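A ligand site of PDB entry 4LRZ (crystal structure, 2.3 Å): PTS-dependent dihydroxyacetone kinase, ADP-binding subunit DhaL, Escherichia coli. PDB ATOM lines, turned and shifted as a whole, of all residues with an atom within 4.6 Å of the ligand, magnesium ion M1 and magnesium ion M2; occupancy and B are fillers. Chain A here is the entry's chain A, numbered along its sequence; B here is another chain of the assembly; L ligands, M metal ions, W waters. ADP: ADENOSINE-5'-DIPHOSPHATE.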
ATOM      1  N   ASP A  31      19.303  11.273   3.366  1.00  0.00           N
ATOM      2  CA  ASP A  31      17.940  10.772   3.351  1.00  0.00           C
ATOM      3  C   ASP A  31      17.182  11.267   4.557  1.00  0.00           C
ATOM      4  O   ASP A  31      15.959  11.201   4.570  1.00  0.00           O
ATOM      5  CB  ASP A  31      17.932   9.216   3.344  1.00  0.00           C
ATOM      6  CG  ASP A  31      16.584   8.578   2.830  1.00  0.00           C
ATOM      7  OD1 ASP A  31      15.950   9.127   1.902  1.00  0.00           O
ATOM      8  OD2 ASP A  31      16.165   7.478   3.337  1.00  0.00           O
ATOM      9  N   ASP A  36      12.874   9.496   4.784  1.00  0.00           N
ATOM     10  CA  ASP A  36      12.633   8.786   6.048  1.00  0.00           C
ATOM     11  C   ASP A  36      13.914   8.306   6.727  1.00  0.00           C
ATOM     12  O   ASP A  36      13.868   7.384   7.561  1.00  0.00           O
ATOM     13  CB  ASP A  36      11.673   7.615   5.799  1.00  0.00           C
ATOM     14  CG  ASP A  36      12.241   6.594   4.817  1.00  0.00           C
ATOM     15  OD1 ASP A  36      11.570   5.578   4.519  1.00  0.00           O
ATOM     16  OD2 ASP A  36      13.387   6.812   4.352  1.00  0.00           O
ATOM     17  N   ALA A  37      15.056   8.890   6.385  1.00  0.00           N
ATOM     18  CA  ALA A  37      16.332   8.591   7.065  1.00  0.00           C
ATOM     19  C   ALA A  37      16.756   7.117   7.042  1.00  0.00           C
ATOM     20  O   ALA A  37      17.162   6.577   8.047  1.00  0.00           O
ATOM     21  CB  ALA A  37      16.286   9.107   8.588  1.00  0.00           C
ATOM     22  N   ASP A  38      16.652   6.440   5.907  1.00  0.00           N
ATOM     23  CA  ASP A  38      16.988   4.990   5.900  1.00  0.00           C
ATOM     24  C   ASP A  38      17.880   4.536   4.713  1.00  0.00           C
ATOM     25  O   ASP A  38      18.362   3.421   4.726  1.00  0.00           O
ATOM     26  CB  ASP A  38      15.702   4.159   5.943  1.00  0.00           C
ATOM     27  CG  ASP A  38      14.864   4.348   4.697  1.00  0.00           C
ATOM     28  OD1 ASP A  38      15.387   4.901   3.711  1.00  0.00           O
ATOM     29  OD2 ASP A  38      13.661   3.953   4.687  1.00  0.00           O
ATOM     30  N   HIS A  39      18.091   5.392   3.715  1.00  0.00           N
ATOM     31  CA  HIS A  39      18.746   4.950   2.471  1.00  0.00           C
ATOM     32  C   HIS A  39      20.111   4.320   2.638  1.00  0.00           C
ATOM     33  O   HIS A  39      20.388   3.266   2.079  1.00  0.00           O
ATOM     34  CB  HIS A  39      18.828   6.057   1.426  1.00  0.00           C
ATOM     35  CG  HIS A  39      19.308   5.578   0.080  1.00  0.00           C
ATOM     36  ND1 HIS A  39      18.577   4.713  -0.708  1.00  0.00           N
ATOM     37  CD2 HIS A  39      20.433   5.862  -0.630  1.00  0.00           C
ATOM     38  CE1 HIS A  39      19.234   4.479  -1.832  1.00  0.00           C
ATOM     39  NE2 HIS A  39      20.359   5.175  -1.812  1.00  0.00           N
ATOM     40  N   ASN A  42      19.614   0.848   4.288  1.00  0.00           N
ATOM     41  CA  ASN A  42      19.017  -0.138   3.392  1.00  0.00           C
ATOM     42  C   ASN A  42      19.972  -0.568   2.268  1.00  0.00           C
ATOM     43  O   ASN A  42      20.049  -1.730   1.953  1.00  0.00           O
ATOM     44  CB  ASN A  42      17.677   0.369   2.846  1.00  0.00           C
ATOM     45  CG  ASN A  42      16.632   0.512   3.953  1.00  0.00           C
ATOM     46  OD1 ASN A  42      15.528   1.022   3.731  1.00  0.00           O
ATOM     47  ND2 ASN A  42      16.990   0.070   5.153  1.00  0.00           N
ATOM     48  N   GLY A  78      14.327  -2.854   0.020  1.00  0.00           N
ATOM     49  CA  GLY A  78      13.089  -2.247   0.458  1.00  0.00           C
ATOM     50  C   GLY A  78      12.893  -0.848  -0.113  1.00  0.00           C
ATOM     51  O   GLY A  78      13.827  -0.261  -0.687  1.00  0.00           O
ATOM     52  N   GLY A  79      11.681  -0.343   0.045  1.00  0.00           N
ATOM     53  CA  GLY A  79      11.290   0.997  -0.329  1.00  0.00           C
ATOM     54  C   GLY A  79      11.346   1.208  -1.836  1.00  0.00           C
ATOM     55  O   GLY A  79      11.267   0.261  -2.621  1.00  0.00           O
ATOM     56  N   ALA A  80      11.498   2.472  -2.223  1.00  0.00           N
ATOM     57  CA  ALA A  80      11.527   2.858  -3.634  1.00  0.00           C
ATOM     58  C   ALA A  80      12.796   2.377  -4.287  1.00  0.00           C
ATOM     59  O   ALA A  80      12.738   1.949  -5.403  1.00  0.00           O
ATOM     60  CB  ALA A  80      11.369   4.346  -3.784  1.00  0.00           C
ATOM     61  N   SER A  81      13.937   2.367  -3.603  1.00  0.00           N
ATOM     62  CA  SER A  81      15.199   2.139  -4.337  1.00  0.00           C
ATOM     63  C   SER A  81      15.506   0.681  -4.601  1.00  0.00           C
ATOM     64  O   SER A  81      16.148   0.354  -5.602  1.00  0.00           O
ATOM     65  CB  SER A  81      16.392   2.840  -3.681  1.00  0.00           C
ATOM     66  OG  SER A  81      16.572   2.343  -2.386  1.00  0.00           O
ATOM     67  N   LEU A  84      14.122  -0.578  -7.853  1.00  0.00           N
ATOM     68  CA  LEU A  84      14.800   0.115  -8.898  1.00  0.00           C
ATOM     69  C   LEU A  84      16.258  -0.389  -9.122  1.00  0.00           C
ATOM     70  O   LEU A  84      16.678  -0.710 -10.256  1.00  0.00           O
ATOM     71  CB  LEU A  84      14.694   1.626  -8.656  1.00  0.00           C
ATOM     72  CG  LEU A  84      13.227   2.156  -8.593  1.00  0.00           C
ATOM     73  CD1 LEU A  84      13.225   3.600  -8.236  1.00  0.00           C
ATOM     74  CD2 LEU A  84      12.420   1.986  -9.895  1.00  0.00           C
ATOM     75  N   GLY A 122      10.021   3.073 -12.786  1.00  0.00           N
ATOM     76  CA  GLY A 122       9.759   4.190 -11.887  1.00  0.00           C
ATOM     77  C   GLY A 122       9.192   5.490 -12.502  1.00  0.00           C
ATOM     78  O   GLY A 122       8.766   6.403 -11.775  1.00  0.00           O
ATOM     79  N   ALA A 124      10.420   8.028 -13.930  1.00  0.00           N
ATOM     80  CA  ALA A 124      11.068   9.290 -13.584  1.00  0.00           C
ATOM     81  C   ALA A 124      11.532  10.013 -14.859  1.00  0.00           C
ATOM     82  O   ALA A 124      11.858   9.377 -15.864  1.00  0.00           O
ATOM     83  CB  ALA A 124      12.227   9.050 -12.626  1.00  0.00           C
ATOM     84  N   THR A 130      15.863  12.320  -8.906  1.00  0.00           N
ATOM     85  CA  THR A 130      15.952  10.900  -8.542  1.00  0.00           C
ATOM     86  C   THR A 130      17.261  10.358  -9.054  1.00  0.00           C
ATOM     87  O   THR A 130      18.051  11.087  -9.616  1.00  0.00           O
ATOM     88  CB  THR A 130      14.815  10.040  -9.151  1.00  0.00           C
ATOM     89  OG1 THR A 130      15.067   9.850 -10.559  1.00  0.00           O
ATOM     90  CG2 THR A 130      13.413  10.642  -8.915  1.00  0.00           C
ATOM     91  N   MET A 131      17.450   9.050  -8.894  1.00  0.00           N
ATOM     92  CA  MET A 131      18.618   8.323  -9.381  1.00  0.00           C
ATOM     93  C   MET A 131      18.727   8.344 -10.913  1.00  0.00           C
ATOM     94  O   MET A 131      19.814   8.092 -11.480  1.00  0.00           O
ATOM     95  CB  MET A 131      18.593   6.888  -8.874  1.00  0.00           C
ATOM     96  CG  MET A 131      17.350   6.086  -9.328  1.00  0.00           C
ATOM     97  SD  MET A 131      17.500   4.283  -9.093  1.00  0.00           S
ATOM     98  CE  MET A 131      17.311   4.093  -7.305  1.00  0.00           C
ATOM     99  N   CYS A 132      17.607   8.605 -11.597  1.00  0.00           N
ATOM    100  CA  CYS A 132      17.636   8.626 -13.079  1.00  0.00           C
ATOM    101  C   CYS A 132      18.328   9.888 -13.585  1.00  0.00           C
ATOM    102  O   CYS A 132      18.807   9.937 -14.734  1.00  0.00           O
ATOM    103  CB  CYS A 132      16.232   8.513 -13.671  1.00  0.00           C
ATOM    104  SG  CYS A 132      15.486   6.937 -13.285  1.00  0.00           S
ATOM    105  N   LYS A 177       9.241  12.955  -7.655  1.00  0.00           N
ATOM    106  CA  LYS A 177       8.982  11.532  -7.386  1.00  0.00           C
ATOM    107  C   LYS A 177       9.470  11.132  -6.011  1.00  0.00           C
ATOM    108  O   LYS A 177      10.363  11.775  -5.446  1.00  0.00           O
ATOM    109  CB  LYS A 177       9.618  10.588  -8.417  1.00  0.00           C
ATOM    110  CG  LYS A 177       9.163  10.792  -9.877  1.00  0.00           C
ATOM    111  CD  LYS A 177       7.881  10.059 -10.217  1.00  0.00           C
ATOM    112  CE  LYS A 177       7.621  10.098 -11.714  1.00  0.00           C
ATOM    113  NZ  LYS A 177       7.381  11.486 -12.173  1.00  0.00           N
ATOM    114  N   GLY A 178       8.870  10.077  -5.480  1.00  0.00           N
ATOM    115  CA  GLY A 178       9.342   9.475  -4.254  1.00  0.00           C
ATOM    116  C   GLY A 178       9.067  10.354  -3.055  1.00  0.00           C
ATOM    117  O   GLY A 178       8.388  11.358  -3.120  1.00  0.00           O
ATOM    118  N   ARG A 179       9.633   9.942  -1.945  1.00  0.00           N
ATOM    119  CA  ARG A 179       9.356  10.507  -0.653  1.00  0.00           C
ATOM    120  C   ARG A 179       9.687  11.993  -0.524  1.00  0.00           C
ATOM    121  O   ARG A 179       9.013  12.737   0.184  1.00  0.00           O
ATOM    122  CB  ARG A 179      10.171   9.723   0.358  1.00  0.00           C
ATOM    123  CG  ARG A 179       9.620   8.342   0.662  1.00  0.00           C
ATOM    124  CD  ARG A 179       8.923   8.526   1.924  1.00  0.00           C
ATOM    125  NE  ARG A 179       9.135   7.451   2.837  1.00  0.00           N
ATOM    126  CZ  ARG A 179       8.380   7.268   3.909  1.00  0.00           C
ATOM    127  NH1 ARG A 179       7.412   8.137   4.175  1.00  0.00           N
ATOM    128  NH2 ARG A 179       8.592   6.218   4.692  1.00  0.00           N
ATOM    129  N   ASP A 192      20.100  14.449  -3.604  1.00  0.00           N
ATOM    130  CA  ASP A 192      19.320  13.190  -3.628  1.00  0.00           C
ATOM    131  C   ASP A 192      20.175  11.973  -3.249  1.00  0.00           C
ATOM    132  O   ASP A 192      21.218  11.757  -3.836  1.00  0.00           O
ATOM    133  CB  ASP A 192      18.726  12.949  -5.003  1.00  0.00           C
ATOM    134  CG  ASP A 192      17.772  11.754  -5.036  1.00  0.00           C
ATOM    135  OD1 ASP A 192      16.694  11.861  -4.360  1.00  0.00           O
ATOM    136  OD2 ASP A 192      18.102  10.705  -5.688  1.00  0.00           O
ATOM    137  N   PRO A 193      19.743  11.172  -2.274  1.00  0.00           N
ATOM    138  CA  PRO A 193      20.517   9.951  -1.881  1.00  0.00           C
ATOM    139  C   PRO A 193      20.552   8.834  -2.932  1.00  0.00           C
ATOM    140  O   PRO A 193      21.580   8.172  -3.097  1.00  0.00           O
ATOM    141  CB  PRO A 193      19.841   9.441  -0.586  1.00  0.00           C
ATOM    142  CG  PRO A 193      18.563  10.242  -0.415  1.00  0.00           C
ATOM    143  CD  PRO A 193      18.595  11.456  -1.380  1.00  0.00           C
ATOM    144  N   GLY A 194      19.458   8.579  -3.629  1.00  0.00           N
ATOM    145  CA  GLY A 194      19.559   7.563  -4.678  1.00  0.00           C
ATOM    146  C   GLY A 194      20.615   7.940  -5.725  1.00  0.00           C
ATOM    147  O   GLY A 194      21.395   7.052  -6.172  1.00  0.00           O
ATOM    148  N   ALA A 195      20.678   9.241  -6.096  1.00  0.00           N
ATOM    149  CA  ALA A 195      21.630   9.723  -7.096  1.00  0.00           C
ATOM    150  C   ALA A 195      23.087   9.608  -6.588  1.00  0.00           C
ATOM    151  O   ALA A 195      23.991   9.276  -7.362  1.00  0.00           O
ATOM    152  CB  ALA A 195      21.333  11.161  -7.527  1.00  0.00           C
ATOM    153  N   GLU B  66       5.031   1.623   5.733  1.00  0.00           N
ATOM    154  CA  GLU B  66       4.990   2.785   4.843  1.00  0.00           C
ATOM    155  C   GLU B  66       3.609   3.036   4.213  1.00  0.00           C
ATOM    156  O   GLU B  66       3.148   4.152   4.247  1.00  0.00           O
ATOM    157  CB  GLU B  66       6.040   2.651   3.733  1.00  0.00           C
ATOM    158  CG  GLU B  66       6.144   3.943   2.883  1.00  0.00           C
ATOM    159  CD  GLU B  66       6.876   3.765   1.541  1.00  0.00           C
ATOM    160  OE1 GLU B  66       6.759   4.696   0.694  1.00  0.00           O
ATOM    161  OE2 GLU B  66       7.567   2.727   1.357  1.00  0.00           O
HETATM  162  PB  ADP L   1      12.495   5.214   0.448  1.00  0.00           P
HETATM  163  O1B ADP L   1      12.763   5.135   1.917  1.00  0.00           O
HETATM  164  O2B ADP L   1      11.330   4.333   0.106  1.00  0.00           O
HETATM  165  O3B ADP L   1      12.417   6.606  -0.075  1.00  0.00           O
HETATM  166  PA  ADP L   1      15.213   4.930  -0.229  1.00  0.00           P
HETATM  167  O1A ADP L   1      15.392   5.884   0.911  1.00  0.00           O
HETATM  168  O2A ADP L   1      16.053   3.680  -0.282  1.00  0.00           O
HETATM  169  O3A ADP L   1      13.693   4.456  -0.289  1.00  0.00           O
HETATM  170  O5' ADP L   1      15.400   5.640  -1.629  1.00  0.00           O
HETATM  171  C5' ADP L   1      15.165   7.021  -1.912  1.00  0.00           C
HETATM  172  C4' ADP L   1      15.654   7.276  -3.331  1.00  0.00           C
HETATM  173  O4' ADP L   1      14.855   6.530  -4.242  1.00  0.00           O
HETATM  174  C3' ADP L   1      15.477   8.732  -3.757  1.00  0.00           C
HETATM  175  O3' ADP L   1      16.657   9.477  -3.388  1.00  0.00           O
HETATM  176  C2' ADP L   1      15.319   8.611  -5.243  1.00  0.00           C
HETATM  177  O2' ADP L   1      16.632   8.665  -5.825  1.00  0.00           O
HETATM  178  C1' ADP L   1      14.811   7.192  -5.506  1.00  0.00           C
HETATM  179  N9  ADP L   1      13.460   7.151  -6.122  1.00  0.00           N
HETATM  180  C8  ADP L   1      12.264   7.295  -5.509  1.00  0.00           C
HETATM  181  N7  ADP L   1      11.249   7.192  -6.423  1.00  0.00           N
HETATM  182  C5  ADP L   1      11.816   7.018  -7.635  1.00  0.00           C
HETATM  183  C6  ADP L   1      11.335   6.831  -9.013  1.00  0.00           C
HETATM  184  N6  ADP L   1      10.033   6.855  -9.328  1.00  0.00           N
HETATM  185  N1  ADP L   1      12.255   6.676  -9.956  1.00  0.00           N
HETATM  186  C2  ADP L   1      13.581   6.662  -9.699  1.00  0.00           C
HETATM  187  N3  ADP L   1      14.081   6.814  -8.460  1.00  0.00           N
HETATM  188  C4  ADP L   1      13.262   6.990  -7.420  1.00  0.00           C
HETATM  189 MG    MG M   1      14.414   6.484   2.548  1.00  0.00          MG
HETATM  190 MG    MG M   2      11.970   3.669   3.557  1.00  0.00          MG
HETATM  191  O   HOH W   1      13.596   7.976   1.579  1.00  0.00           O
HETATM  192  O   HOH W   2      14.955   1.562   1.235  1.00  0.00           O
HETATM  193  O   HOH W   3      12.864   2.275   2.682  1.00  0.00           O
HETATM  194  O   HOH W   4      12.167   5.987 -12.635  1.00  0.00           O
HETATM  195  O   HOH W   5       8.936   6.309  -5.501  1.00  0.00           O
HETATM  196  O   HOH W   6      11.414   7.754  -2.286  1.00  0.00           O
HETATM  197  O   HOH W   7      10.340   3.987   2.427  1.00  0.00           O
HETATM  198  O   HOH W   8      14.978  10.770  -0.761  1.00  0.00           O
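N of Gly 194 sits at hydrogen-bond distance from O3' of the ligand, 3.0 Å away. The backbone NH of Met 131 lies within hydrogen-bond range of an oxygen (O2') of the ligand (3.2 Å). O2A of the ligand lies within hydrogen-bond range of ND1 of His 39 (2.8 Å). O of Gly 122 lies within hydrogen-bond range of N6 of the ligand, 2.8 Å away. An oxygen (O2B) of the ligand is in hydrogen-bond range of the backbone NH of Ala 80. O2' of the ligand sits at hydrogen-bond distance from OD2 of Asp 192. The side-chain hydroxyl of Ser 81 lies within hydrogen-bond range of an oxygen (O2A) of the ligand, at 2.5 Å.
The side-chain carboxylate (OD1) of Asp 36 lies close to the guanidinium group (NH2) of Arg 179 (3.1 Å). The side-chain carboxylate of Asp 192 lies within hydrogen-bond range of the backbone NH of Ala 195 (3.0 Å). The side-chain carboxylate (OD2) of Asp 31 lies close to the backbone NH (N) of His 39 (2.9 Å). OG1 of Thr 130 sits at hydrogen-bond distance from N of Cys 132, at 3.0 Å. A ring nitrogen (NE2) of His 39 sits at hydrogen-bond distance from the backbone carbonyl oxygen (O) of Pro 193 (3.5 Å). OD2 of Asp 192 lies within hydrogen-bond range of N of Gly 194. The backbone carbonyl oxygen (O) of Asp 31 sits at hydrogen-bond distance from the backbone NH (N) of Ala 37 (3.1 Å).
Gly 79 touches the ligand. CD1 of Leu 84 touches N3 of the ligand (3.3 Å). Ala 124 touches the ligand (CB to N1, 3.6 Å). Thr 130 touches the ligand (CB to N3, 3.4 Å). Lys 177 touches the ligand. Gly 178 touches the ligand (CA to N7, 3.7 Å). Arg 179 touches the ligand. CD of Pro 193 touches O3' of the ligand, at 3.4 Å. Hydrophobic or aromatic side chains within 4 Å of the ligand: His 39, Ala 80, Leu 84, Ala 124, Met 131 and Pro 193.
Two residues have an atom within 4 Å of magnesium ion M2: Asp 36 and Asp 38.
Magnesium ion M1 is bound by water W1, an oxygen (O1A) of the ligand, the side-chain carboxylate (OD2) of Asp 36, the side-chain carboxylate (OD2) of Asp 31, the side-chain carboxylate (OD1) of Asp 38 and an oxygen (O1B) of the ligand. Magnesium ion M1 has six donor atoms within binding distance.
Magnesium ion M2 is bound by water W3, water W7, the side-chain carboxylate (OD2) of Asp 38, the side-chain carboxylate (OD1) of Asp 36 and an oxygen (O1B) of the ligand.
Water W1 lies within hydrogen-bond range of O3B of the ligand (2.5 Å) and OD1 of Asp 31 (2.6 Å). Water W7 lies within hydrogen-bond range of an oxygen (O2B) of the ligand (2.5 Å) and the side-chain carboxylate (OE2) of Glu 66 of chain B (3.2 Å). Water W6 bridges an oxygen (O3B) of the ligand and the backbone NH (N) of Arg 179. Water W4 lies within hydrogen-bond range of a nitrogen (N1) of the ligand, the backbone NH of Ala 124 and the side-chain sulfur of Cys 132. Water W2 lies within hydrogen-bond range of OD1 of Asn 42 (2.6 Å), O2A of the ligand (2.8 Å) and O of Gly 78 (2.9 Å). Water W8 lies within hydrogen-bond range of the side-chain carboxylate (OD1) of Asp 31 and an oxygen (O3') of the ligand.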
